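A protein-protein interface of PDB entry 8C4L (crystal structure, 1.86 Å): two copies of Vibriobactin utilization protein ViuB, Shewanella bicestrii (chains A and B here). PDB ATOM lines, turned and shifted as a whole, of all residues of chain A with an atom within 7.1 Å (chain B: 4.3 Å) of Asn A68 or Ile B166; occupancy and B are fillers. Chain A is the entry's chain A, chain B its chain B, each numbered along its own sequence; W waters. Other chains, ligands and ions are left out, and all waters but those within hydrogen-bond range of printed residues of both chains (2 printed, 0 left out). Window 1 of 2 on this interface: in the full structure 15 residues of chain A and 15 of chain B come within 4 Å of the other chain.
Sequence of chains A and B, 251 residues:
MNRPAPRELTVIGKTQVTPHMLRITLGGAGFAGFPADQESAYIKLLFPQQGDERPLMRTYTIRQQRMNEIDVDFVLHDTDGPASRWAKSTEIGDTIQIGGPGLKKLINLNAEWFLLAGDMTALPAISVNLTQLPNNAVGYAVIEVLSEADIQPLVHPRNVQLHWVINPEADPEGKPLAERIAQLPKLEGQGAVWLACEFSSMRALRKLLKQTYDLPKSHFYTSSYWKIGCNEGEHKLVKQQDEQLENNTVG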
ATOM      1  N   LEU A   9      25.267 -25.883  -5.642  1.00  0.00           N
ATOM      2  CA  LEU A   9      24.260 -26.449  -4.765  1.00  0.00           C
ATOM      3  C   LEU A   9      23.624 -27.662  -5.426  1.00  0.00           C
ATOM      4  O   LEU A   9      23.582 -27.760  -6.652  1.00  0.00           O
ATOM      5  CB  LEU A   9      23.196 -25.403  -4.452  1.00  0.00           C
ATOM      6  CG  LEU A   9      23.677 -24.140  -3.715  1.00  0.00           C
ATOM      7  CD1 LEU A   9      22.504 -23.258  -3.350  1.00  0.00           C
ATOM      8  CD2 LEU A   9      24.426 -24.504  -2.463  1.00  0.00           C
ATOM      9  N   THR A  10      23.104 -28.571  -4.602  1.00  0.00           N
ATOM     10  CA  THR A  10      22.468 -29.797  -5.061  1.00  0.00           C
ATOM     11  C   THR A  10      20.955 -29.689  -4.927  1.00  0.00           C
ATOM     12  O   THR A  10      20.436 -29.172  -3.928  1.00  0.00           O
ATOM     13  CB  THR A  10      22.993 -31.025  -4.269  1.00  0.00           C
ATOM     14  OG1 THR A  10      24.405 -31.126  -4.425  1.00  0.00           O
ATOM     15  CG2 THR A  10      22.393 -32.321  -4.773  1.00  0.00           C
ATOM     16  N   VAL A  11      20.252 -30.156  -5.960  1.00  0.00           N
ATOM     17  CA  VAL A  11      18.805 -30.290  -5.892  1.00  0.00           C
ATOM     18  C   VAL A  11      18.463 -31.382  -4.888  1.00  0.00           C
ATOM     19  O   VAL A  11      18.842 -32.550  -5.063  1.00  0.00           O
ATOM     20  CB  VAL A  11      18.216 -30.603  -7.272  1.00  0.00           C
ATOM     21  CG1 VAL A  11      16.709 -30.771  -7.155  1.00  0.00           C
ATOM     22  CG2 VAL A  11      18.531 -29.473  -8.224  1.00  0.00           C
ATOM     23  N   ILE A  12      17.769 -31.002  -3.808  1.00  0.00           N
ATOM     24  CA  ILE A  12      17.431 -31.950  -2.754  1.00  0.00           C
ATOM     25  C   ILE A  12      15.933 -32.052  -2.510  1.00  0.00           C
ATOM     26  O   ILE A  12      15.519 -32.746  -1.589  1.00  0.00           O
ATOM     27  CB  ILE A  12      18.174 -31.628  -1.442  1.00  0.00           C
ATOM     28  CG1 ILE A  12      17.907 -30.204  -0.977  1.00  0.00           C
ATOM     29  CG2 ILE A  12      19.713 -31.900  -1.619  1.00  0.00           C
ATOM     30  CD1 ILE A  12      18.656 -29.907   0.295  1.00  0.00           C
ATOM     31  N   THR A  25      14.256 -27.149  -3.955  1.00  0.00           N
ATOM     32  CA  THR A  25      15.070 -26.976  -2.763  1.00  0.00           C
ATOM     33  C   THR A  25      16.539 -27.257  -3.104  1.00  0.00           C
ATOM     34  O   THR A  25      16.868 -28.267  -3.741  1.00  0.00           O
ATOM     35  CB  THR A  25      14.601 -27.901  -1.638  1.00  0.00           C
ATOM     36  OG1 THR A  25      13.219 -27.664  -1.339  1.00  0.00           O
ATOM     37  CG2 THR A  25      15.464 -27.657  -0.379  1.00  0.00           C
ATOM     38  N   LEU A  26      17.412 -26.348  -2.709  1.00  0.00           N
ATOM     39  CA  LEU A  26      18.838 -26.422  -3.020  1.00  0.00           C
ATOM     40  C   LEU A  26      19.659 -26.357  -1.749  1.00  0.00           C
ATOM     41  O   LEU A  26      19.404 -25.503  -0.896  1.00  0.00           O
ATOM     42  CB  LEU A  26      19.256 -25.262  -3.928  1.00  0.00           C
ATOM     43  CG  LEU A  26      18.543 -25.155  -5.297  1.00  0.00           C
ATOM     44  CD1 LEU A  26      18.820 -23.843  -5.877  1.00  0.00           C
ATOM     45  CD2 LEU A  26      19.042 -26.212  -6.285  1.00  0.00           C
ATOM     46  N   GLY A  27      20.651 -27.234  -1.628  1.00  0.00           N
ATOM     47  CA  GLY A  27      21.575 -27.110  -0.519  1.00  0.00           C
ATOM     48  C   GLY A  27      22.809 -27.964  -0.659  1.00  0.00           C
ATOM     49  O   GLY A  27      23.176 -28.342  -1.761  1.00  0.00           O
ATOM     50  N   GLY A  28      23.387 -28.376   0.448  1.00  0.00           N
ATOM     51  CA  GLY A  28      24.605 -29.150   0.402  1.00  0.00           C
ATOM     52  C   GLY A  28      25.820 -28.346   0.781  1.00  0.00           C
ATOM     53  O   GLY A  28      25.740 -27.235   1.318  1.00  0.00           O
ATOM     54  N   ALA A  29      26.976 -28.941   0.482  1.00  0.00           N
ATOM     55  CA  ALA A  29      28.247 -28.422   0.982  1.00  0.00           C
ATOM     56  C   ALA A  29      28.549 -27.044   0.428  1.00  0.00           C
ATOM     57  O   ALA A  29      29.153 -26.228   1.117  1.00  0.00           O
ATOM     58  CB  ALA A  29      29.379 -29.376   0.620  1.00  0.00           C
ATOM     59  N   GLY A  30      28.111 -26.752  -0.795  1.00  0.00           N
ATOM     60  CA  GLY A  30      28.311 -25.440  -1.367  1.00  0.00           C
ATOM     61  C   GLY A  30      27.601 -24.344  -0.625  1.00  0.00           C
ATOM     62  O   GLY A  30      27.875 -23.167  -0.887  1.00  0.00           O
ATOM     63  N   PHE A  31      26.677 -24.695   0.277  1.00  0.00           N
ATOM     64  CA  PHE A  31      25.890 -23.713   1.027  1.00  0.00           C
ATOM     65  C   PHE A  31      26.644 -23.132   2.213  1.00  0.00           C
ATOM     66  O   PHE A  31      26.216 -22.120   2.776  1.00  0.00           O
ATOM     67  CB  PHE A  31      24.568 -24.352   1.495  1.00  0.00           C
ATOM     68  CG  PHE A  31      23.535 -23.351   1.852  1.00  0.00           C
ATOM     69  CD1 PHE A  31      22.867 -22.682   0.854  1.00  0.00           C
ATOM     70  CD2 PHE A  31      23.236 -23.056   3.177  1.00  0.00           C
ATOM     71  CE1 PHE A  31      21.910 -21.723   1.150  1.00  0.00           C
ATOM     72  CE2 PHE A  31      22.265 -22.117   3.486  1.00  0.00           C
ATOM     73  CZ  PHE A  31      21.599 -21.454   2.465  1.00  0.00           C
ATOM     74  N   ALA A  32      27.734 -23.761   2.624  1.00  0.00           N
ATOM     75  CA  ALA A  32      28.470 -23.324   3.794  1.00  0.00           C
ATOM     76  C   ALA A  32      28.823 -21.856   3.669  1.00  0.00           C
ATOM     77  O   ALA A  32      29.276 -21.396   2.619  1.00  0.00           O
ATOM     78  CB  ALA A  32      29.723 -24.179   3.967  1.00  0.00           C
ATOM     79  N   GLY A  33      28.542 -21.104   4.721  1.00  0.00           N
ATOM     80  CA  GLY A  33      28.863 -19.701   4.742  1.00  0.00           C
ATOM     81  C   GLY A  33      27.783 -18.813   4.170  1.00  0.00           C
ATOM     82  O   GLY A  33      27.890 -17.588   4.289  1.00  0.00           O
ATOM     83  N   GLN A  65      14.345 -19.983   3.511  1.00  0.00           N
ATOM     84  CA  GLN A  65      15.724 -20.299   3.853  1.00  0.00           C
ATOM     85  C   GLN A  65      15.741 -21.031   5.176  1.00  0.00           C
ATOM     86  O   GLN A  65      15.129 -20.566   6.143  1.00  0.00           O
ATOM     87  CB  GLN A  65      16.545 -19.013   3.971  1.00  0.00           C
ATOM     88  CG  GLN A  65      18.001 -19.266   4.358  1.00  0.00           C
ATOM     89  CD  GLN A  65      18.835 -18.054   4.184  1.00  0.00           C
ATOM     90  OE1 GLN A  65      18.372 -17.039   3.654  1.00  0.00           O
ATOM     91  NE2 GLN A  65      20.080 -18.130   4.645  1.00  0.00           N
ATOM     92  N   ARG A  66      16.469 -22.144   5.224  1.00  0.00           N
ATOM     93  CA  ARG A  66      16.634 -22.953   6.427  1.00  0.00           C
ATOM     94  C   ARG A  66      18.143 -23.108   6.718  1.00  0.00           C
ATOM     95  O   ARG A  66      18.988 -22.470   6.085  1.00  0.00           O
ATOM     96  CB  ARG A  66      15.899 -24.295   6.277  1.00  0.00           C
ATOM     97  CG  ARG A  66      14.374 -24.130   6.150  1.00  0.00           C
ATOM     98  CD  ARG A  66      13.691 -25.417   5.845  1.00  0.00           C
ATOM     99  NE  ARG A  66      14.014 -25.913   4.518  1.00  0.00           N
ATOM    100  CZ  ARG A  66      13.415 -25.539   3.395  1.00  0.00           C
ATOM    101  NH1 ARG A  66      12.473 -24.602   3.377  1.00  0.00           N
ATOM    102  NH2 ARG A  66      13.749 -26.136   2.260  1.00  0.00           N
ATOM    103  N   MET A  67      18.478 -23.938   7.701  1.00  0.00           N
ATOM    104  CA  MET A  67      19.863 -23.998   8.183  1.00  0.00           C
ATOM    105  C   MET A  67      20.871 -24.246   7.052  1.00  0.00           C
ATOM    106  O   MET A  67      21.909 -23.585   6.977  1.00  0.00           O
ATOM    107  CB  MET A  67      19.994 -25.094   9.239  1.00  0.00           C
ATOM    108  CG  MET A  67      19.404 -24.778  10.602  1.00  0.00           C
ATOM    109  SD  MET A  67      19.409 -26.218  11.717  1.00  0.00           S
ATOM    110  CE  MET A  67      21.082 -26.943  11.476  1.00  0.00           C
ATOM    111  N   ASN A  68      20.601 -25.214   6.183  1.00  0.00           N
ATOM    112  CA  ASN A  68      21.576 -25.620   5.176  1.00  0.00           C
ATOM    113  C   ASN A  68      20.958 -25.701   3.781  1.00  0.00           C
ATOM    114  O   ASN A  68      21.389 -26.512   2.961  1.00  0.00           O
ATOM    115  CB  ASN A  68      22.223 -26.949   5.574  1.00  0.00           C
ATOM    116  CG  ASN A  68      23.692 -27.067   5.096  1.00  0.00           C
ATOM    117  OD1 ASN A  68      24.456 -26.104   5.200  1.00  0.00           O
ATOM    118  ND2 ASN A  68      24.090 -28.253   4.579  1.00  0.00           N
ATOM    119  N   GLU A  69      19.907 -24.926   3.503  1.00  0.00           N
ATOM    120  CA  GLU A  69      19.233 -25.024   2.203  1.00  0.00           C
ATOM    121  C   GLU A  69      18.348 -23.790   1.979  1.00  0.00           C
ATOM    122  O   GLU A  69      17.975 -23.095   2.926  1.00  0.00           O
ATOM    123  CB  GLU A  69      18.415 -26.336   2.100  1.00  0.00           C
ATOM    124  CG  GLU A  69      17.315 -26.424   3.141  1.00  0.00           C
ATOM    125  CD  GLU A  69      16.867 -27.827   3.457  1.00  0.00           C
ATOM    126  OE1 GLU A  69      17.710 -28.741   3.516  1.00  0.00           O
ATOM    127  OE2 GLU A  69      15.651 -28.021   3.661  1.00  0.00           O
ATOM    128  N   ILE A  70      18.039 -23.520   0.699  1.00  0.00           N
ATOM    129  CA  ILE A  70      17.038 -22.548   0.275  1.00  0.00           C
ATOM    130  C   ILE A  70      16.043 -23.209  -0.666  1.00  0.00           C
ATOM    131  O   ILE A  70      16.345 -24.235  -1.286  1.00  0.00           O
ATOM    132  CB  ILE A  70      17.658 -21.316  -0.423  1.00  0.00           C
ATOM    133  CG1 ILE A  70      18.611 -21.716  -1.563  1.00  0.00           C
ATOM    134  CG2 ILE A  70      18.391 -20.455   0.583  1.00  0.00           C
ATOM    135  CD1 ILE A  70      18.983 -20.501  -2.474  1.00  0.00           C
ATOM    136  N   VAL B 145      20.687 -36.594   5.925  1.00  0.00           N
ATOM    137  CA  VAL B 145      21.914 -37.319   5.640  1.00  0.00           C
ATOM    138  C   VAL B 145      23.094 -36.389   5.881  1.00  0.00           C
ATOM    139  O   VAL B 145      22.964 -35.168   5.874  1.00  0.00           O
ATOM    140  CB  VAL B 145      21.951 -37.874   4.203  1.00  0.00           C
ATOM    141  CG1 VAL B 145      20.872 -38.904   4.002  1.00  0.00           C
ATOM    142  CG2 VAL B 145      21.810 -36.756   3.188  1.00  0.00           C
ATOM    143  N   LEU B 146      24.264 -36.999   6.081  1.00  0.00           N
ATOM    144  CA  LEU B 146      25.473 -36.261   6.442  1.00  0.00           C
ATOM    145  C   LEU B 146      26.068 -35.473   5.263  1.00  0.00           C
ATOM    146  O   LEU B 146      26.719 -34.444   5.475  1.00  0.00           O
ATOM    147  CB  LEU B 146      26.510 -37.244   7.006  1.00  0.00           C
ATOM    148  CG  LEU B 146      26.172 -37.869   8.366  1.00  0.00           C
ATOM    149  CD1 LEU B 146      27.128 -39.015   8.717  1.00  0.00           C
ATOM    150  CD2 LEU B 146      26.222 -36.793   9.436  1.00  0.00           C
ATOM    151  N   SER B 147      25.858 -35.910   4.028  1.00  0.00           N
ATOM    152  CA  SER B 147      26.457 -35.222   2.891  1.00  0.00           C
ATOM    153  C   SER B 147      25.631 -35.532   1.656  1.00  0.00           C
ATOM    154  O   SER B 147      24.843 -36.477   1.650  1.00  0.00           O
ATOM    155  CB  SER B 147      27.895 -35.674   2.655  1.00  0.00           C
ATOM    156  OG  SER B 147      27.918 -36.953   2.047  1.00  0.00           O
ATOM    157  N   GLU B 148      25.812 -34.735   0.604  1.00  0.00           N
ATOM    158  CA  GLU B 148      25.044 -35.014  -0.606  1.00  0.00           C
ATOM    159  C   GLU B 148      25.369 -36.388  -1.179  1.00  0.00           C
ATOM    160  O   GLU B 148      24.540 -36.976  -1.879  1.00  0.00           O
ATOM    161  CB  GLU B 148      25.223 -33.908  -1.661  1.00  0.00           C
ATOM    162  CG  GLU B 148      26.551 -33.289  -1.790  1.00  0.00           C
ATOM    163  CD  GLU B 148      26.501 -31.789  -1.497  1.00  0.00           C
ATOM    164  OE1 GLU B 148      25.987 -30.981  -2.320  1.00  0.00           O
ATOM    165  OE2 GLU B 148      26.979 -31.417  -0.416  1.00  0.00           O
ATOM    166  N   TRP B 164      15.541 -34.513   0.768  1.00  0.00           N
ATOM    167  CA  TRP B 164      16.783 -34.783   1.459  1.00  0.00           C
ATOM    168  C   TRP B 164      17.230 -33.521   2.170  1.00  0.00           C
ATOM    169  O   TRP B 164      17.189 -32.422   1.594  1.00  0.00           O
ATOM    170  CB  TRP B 164      17.863 -35.273   0.491  1.00  0.00           C
ATOM    171  CG  TRP B 164      17.458 -36.537  -0.218  1.00  0.00           C
ATOM    172  CD1 TRP B 164      16.786 -36.633  -1.383  1.00  0.00           C
ATOM    173  CD2 TRP B 164      17.688 -37.879   0.229  1.00  0.00           C
ATOM    174  NE1 TRP B 164      16.598 -37.961  -1.716  1.00  0.00           N
ATOM    175  CE2 TRP B 164      17.135 -38.740  -0.728  1.00  0.00           C
ATOM    176  CE3 TRP B 164      18.312 -38.425   1.338  1.00  0.00           C
ATOM    177  CZ2 TRP B 164      17.206 -40.105  -0.621  1.00  0.00           C
ATOM    178  CZ3 TRP B 164      18.375 -39.782   1.451  1.00  0.00           C
ATOM    179  CH2 TRP B 164      17.821 -40.612   0.482  1.00  0.00           C
ATOM    180  N   VAL B 165      17.588 -33.680   3.440  1.00  0.00           N
ATOM    181  CA  VAL B 165      18.126 -32.598   4.257  1.00  0.00           C
ATOM    182  C   VAL B 165      19.574 -32.944   4.548  1.00  0.00           C
ATOM    183  O   VAL B 165      19.872 -34.012   5.101  1.00  0.00           O
ATOM    184  CB  VAL B 165      17.328 -32.428   5.553  1.00  0.00           C
ATOM    185  CG1 VAL B 165      17.971 -31.371   6.400  1.00  0.00           C
ATOM    186  CG2 VAL B 165      15.873 -32.072   5.243  1.00  0.00           C
ATOM    187  N   ILE B 166      20.475 -32.070   4.167  1.00  0.00           N
ATOM    188  CA  ILE B 166      21.896 -32.368   4.268  1.00  0.00           C
ATOM    189  C   ILE B 166      22.389 -31.633   5.479  1.00  0.00           C
ATOM    190  O   ILE B 166      22.323 -30.407   5.524  1.00  0.00           O
ATOM    191  CB  ILE B 166      22.646 -31.986   2.985  1.00  0.00           C
ATOM    192  CG1 ILE B 166      22.143 -32.905   1.853  1.00  0.00           C
ATOM    193  CG2 ILE B 166      24.163 -32.196   3.135  1.00  0.00           C
ATOM    194  CD1 ILE B 166      22.550 -32.442   0.549  1.00  0.00           C
ATOM    195  N   ASN B 167      22.816 -32.383   6.480  1.00  0.00           N
ATOM    196  CA  ASN B 167      23.207 -31.815   7.758  1.00  0.00           C
ATOM    197  C   ASN B 167      24.450 -32.554   8.248  1.00  0.00           C
ATOM    198  O   ASN B 167      24.335 -33.693   8.703  1.00  0.00           O
ATOM    199  CB  ASN B 167      22.083 -31.932   8.789  1.00  0.00           C
ATOM    200  CG  ASN B 167      22.500 -31.376  10.126  1.00  0.00           C
ATOM    201  OD1 ASN B 167      23.341 -30.476  10.183  1.00  0.00           O
ATOM    202  ND2 ASN B 167      21.980 -31.946  11.212  1.00  0.00           N
ATOM    203  N   PRO B 168      25.644 -31.946   8.198  1.00  0.00           N
ATOM    204  CA  PRO B 168      26.872 -32.711   8.467  1.00  0.00           C
ATOM    205  C   PRO B 168      27.064 -33.072   9.919  1.00  0.00           C
ATOM    206  O   PRO B 168      27.931 -33.898  10.221  1.00  0.00           O
ATOM    207  CB  PRO B 168      27.990 -31.769   8.018  1.00  0.00           C
ATOM    208  CG  PRO B 168      27.318 -30.602   7.394  1.00  0.00           C
ATOM    209  CD  PRO B 168      25.950 -30.532   7.943  1.00  0.00           C
HETATM  210  O   HOH W   1      26.783 -28.207  -2.658  1.00  0.00           O
HETATM  211  O   HOH W   2      20.159 -29.323   3.266  1.00  0.00           O
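No position is printed for both chains.
Printed residues of chain A that touch a printed residue of chain B: Thr A10, Ile A12, Gly A27, Gly A28, Ala A29, Asn A68 and Glu A69.
Hydrophobic or aromatic side chains of chain A that line the printed part of chain B: Ile A12 and Ala A29.
Of the 9 printed residues of chain B, 4 touch a printed residue of chain A.
Hydrophobic or aromatic side chains of chain B that line the printed part of chain A: Val B165 and Ile B166.
Among the printed residues, 9 pairs touch across the chains.
OE1 of Glu B148 lies within hydrogen-bond range of OG1 of Thr A10.
The backbone NH of Trp B164 is in hydrogen-bond range of the backbone carbonyl oxygen of Ile A12 (2.9 Å).
N of Ala A29 sits at hydrogen-bond distance from OE2 of Glu B148 (2.6 Å).
The backbone carbonyl oxygen (O) of Ile B166 lies within hydrogen-bond range of the side-chain amide nitrogen (ND2) of Asn A68, at 2.9 Å.
Ile B166 touches just these residues of chain A: Ile A12, Gly A28 and Asn A68.
Of the printed residues of chain B, Glu A69 touches Val B165 (3.9 Å).
Of the printed residues of chain B, Thr A10 touches Glu B148 (2.6 Å).
Ser B147 touches none of the printed residues of chain A.
Met A67 touches none of the printed residues of chain B.
The nearest residue of chain A that does not touch Ile B166 is Glu A69 (4.4 Å).
The nearest printed residue of chain B that does not touch Glu A69 is Trp B164 (4.2 Å).
The backbone carbonyl oxygen of Gly A27 is in hydrogen-bond range of the backbone NH of Thr A10 (2.9 Å).
N of Ile A12 lies within hydrogen-bond range of O of Thr A25 (2.9 Å).
The guanidinium group (NE) of Arg A66 is in salt-bridge range of the side-chain carboxylate (OE2) of Glu A69, at 2.8 Å.
N of Val B145 is in hydrogen-bond range of O of Val B165 (2.8 Å).
CG2 of Ile A12 touches CD1 of Ile B166, at 3.6 Å.
Gly A27 touches Glu B148 (O to OE1, 3.9 Å).
OE2 of Glu B148 touches CA of Gly A28 (3.4 Å).
Ile B166 touches Gly A28 (CD1 to CA, 3.9 Å).
Glu A69 touches Val B165.
Water W2 lies within hydrogen-bond range of the side-chain carboxylate of Glu A69 (2.5 Å), the backbone NH of Ile B166 (2.9 Å) and the backbone carbonyl oxygen of Asn A68 (3.1 Å).
Water W1 lies within hydrogen-bond range of the backbone NH of Gly A30 (2.7 Å), the side-chain carboxylate of Glu B148 (2.9 Å) and the backbone NH of Ala A29 (3.2 Å).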
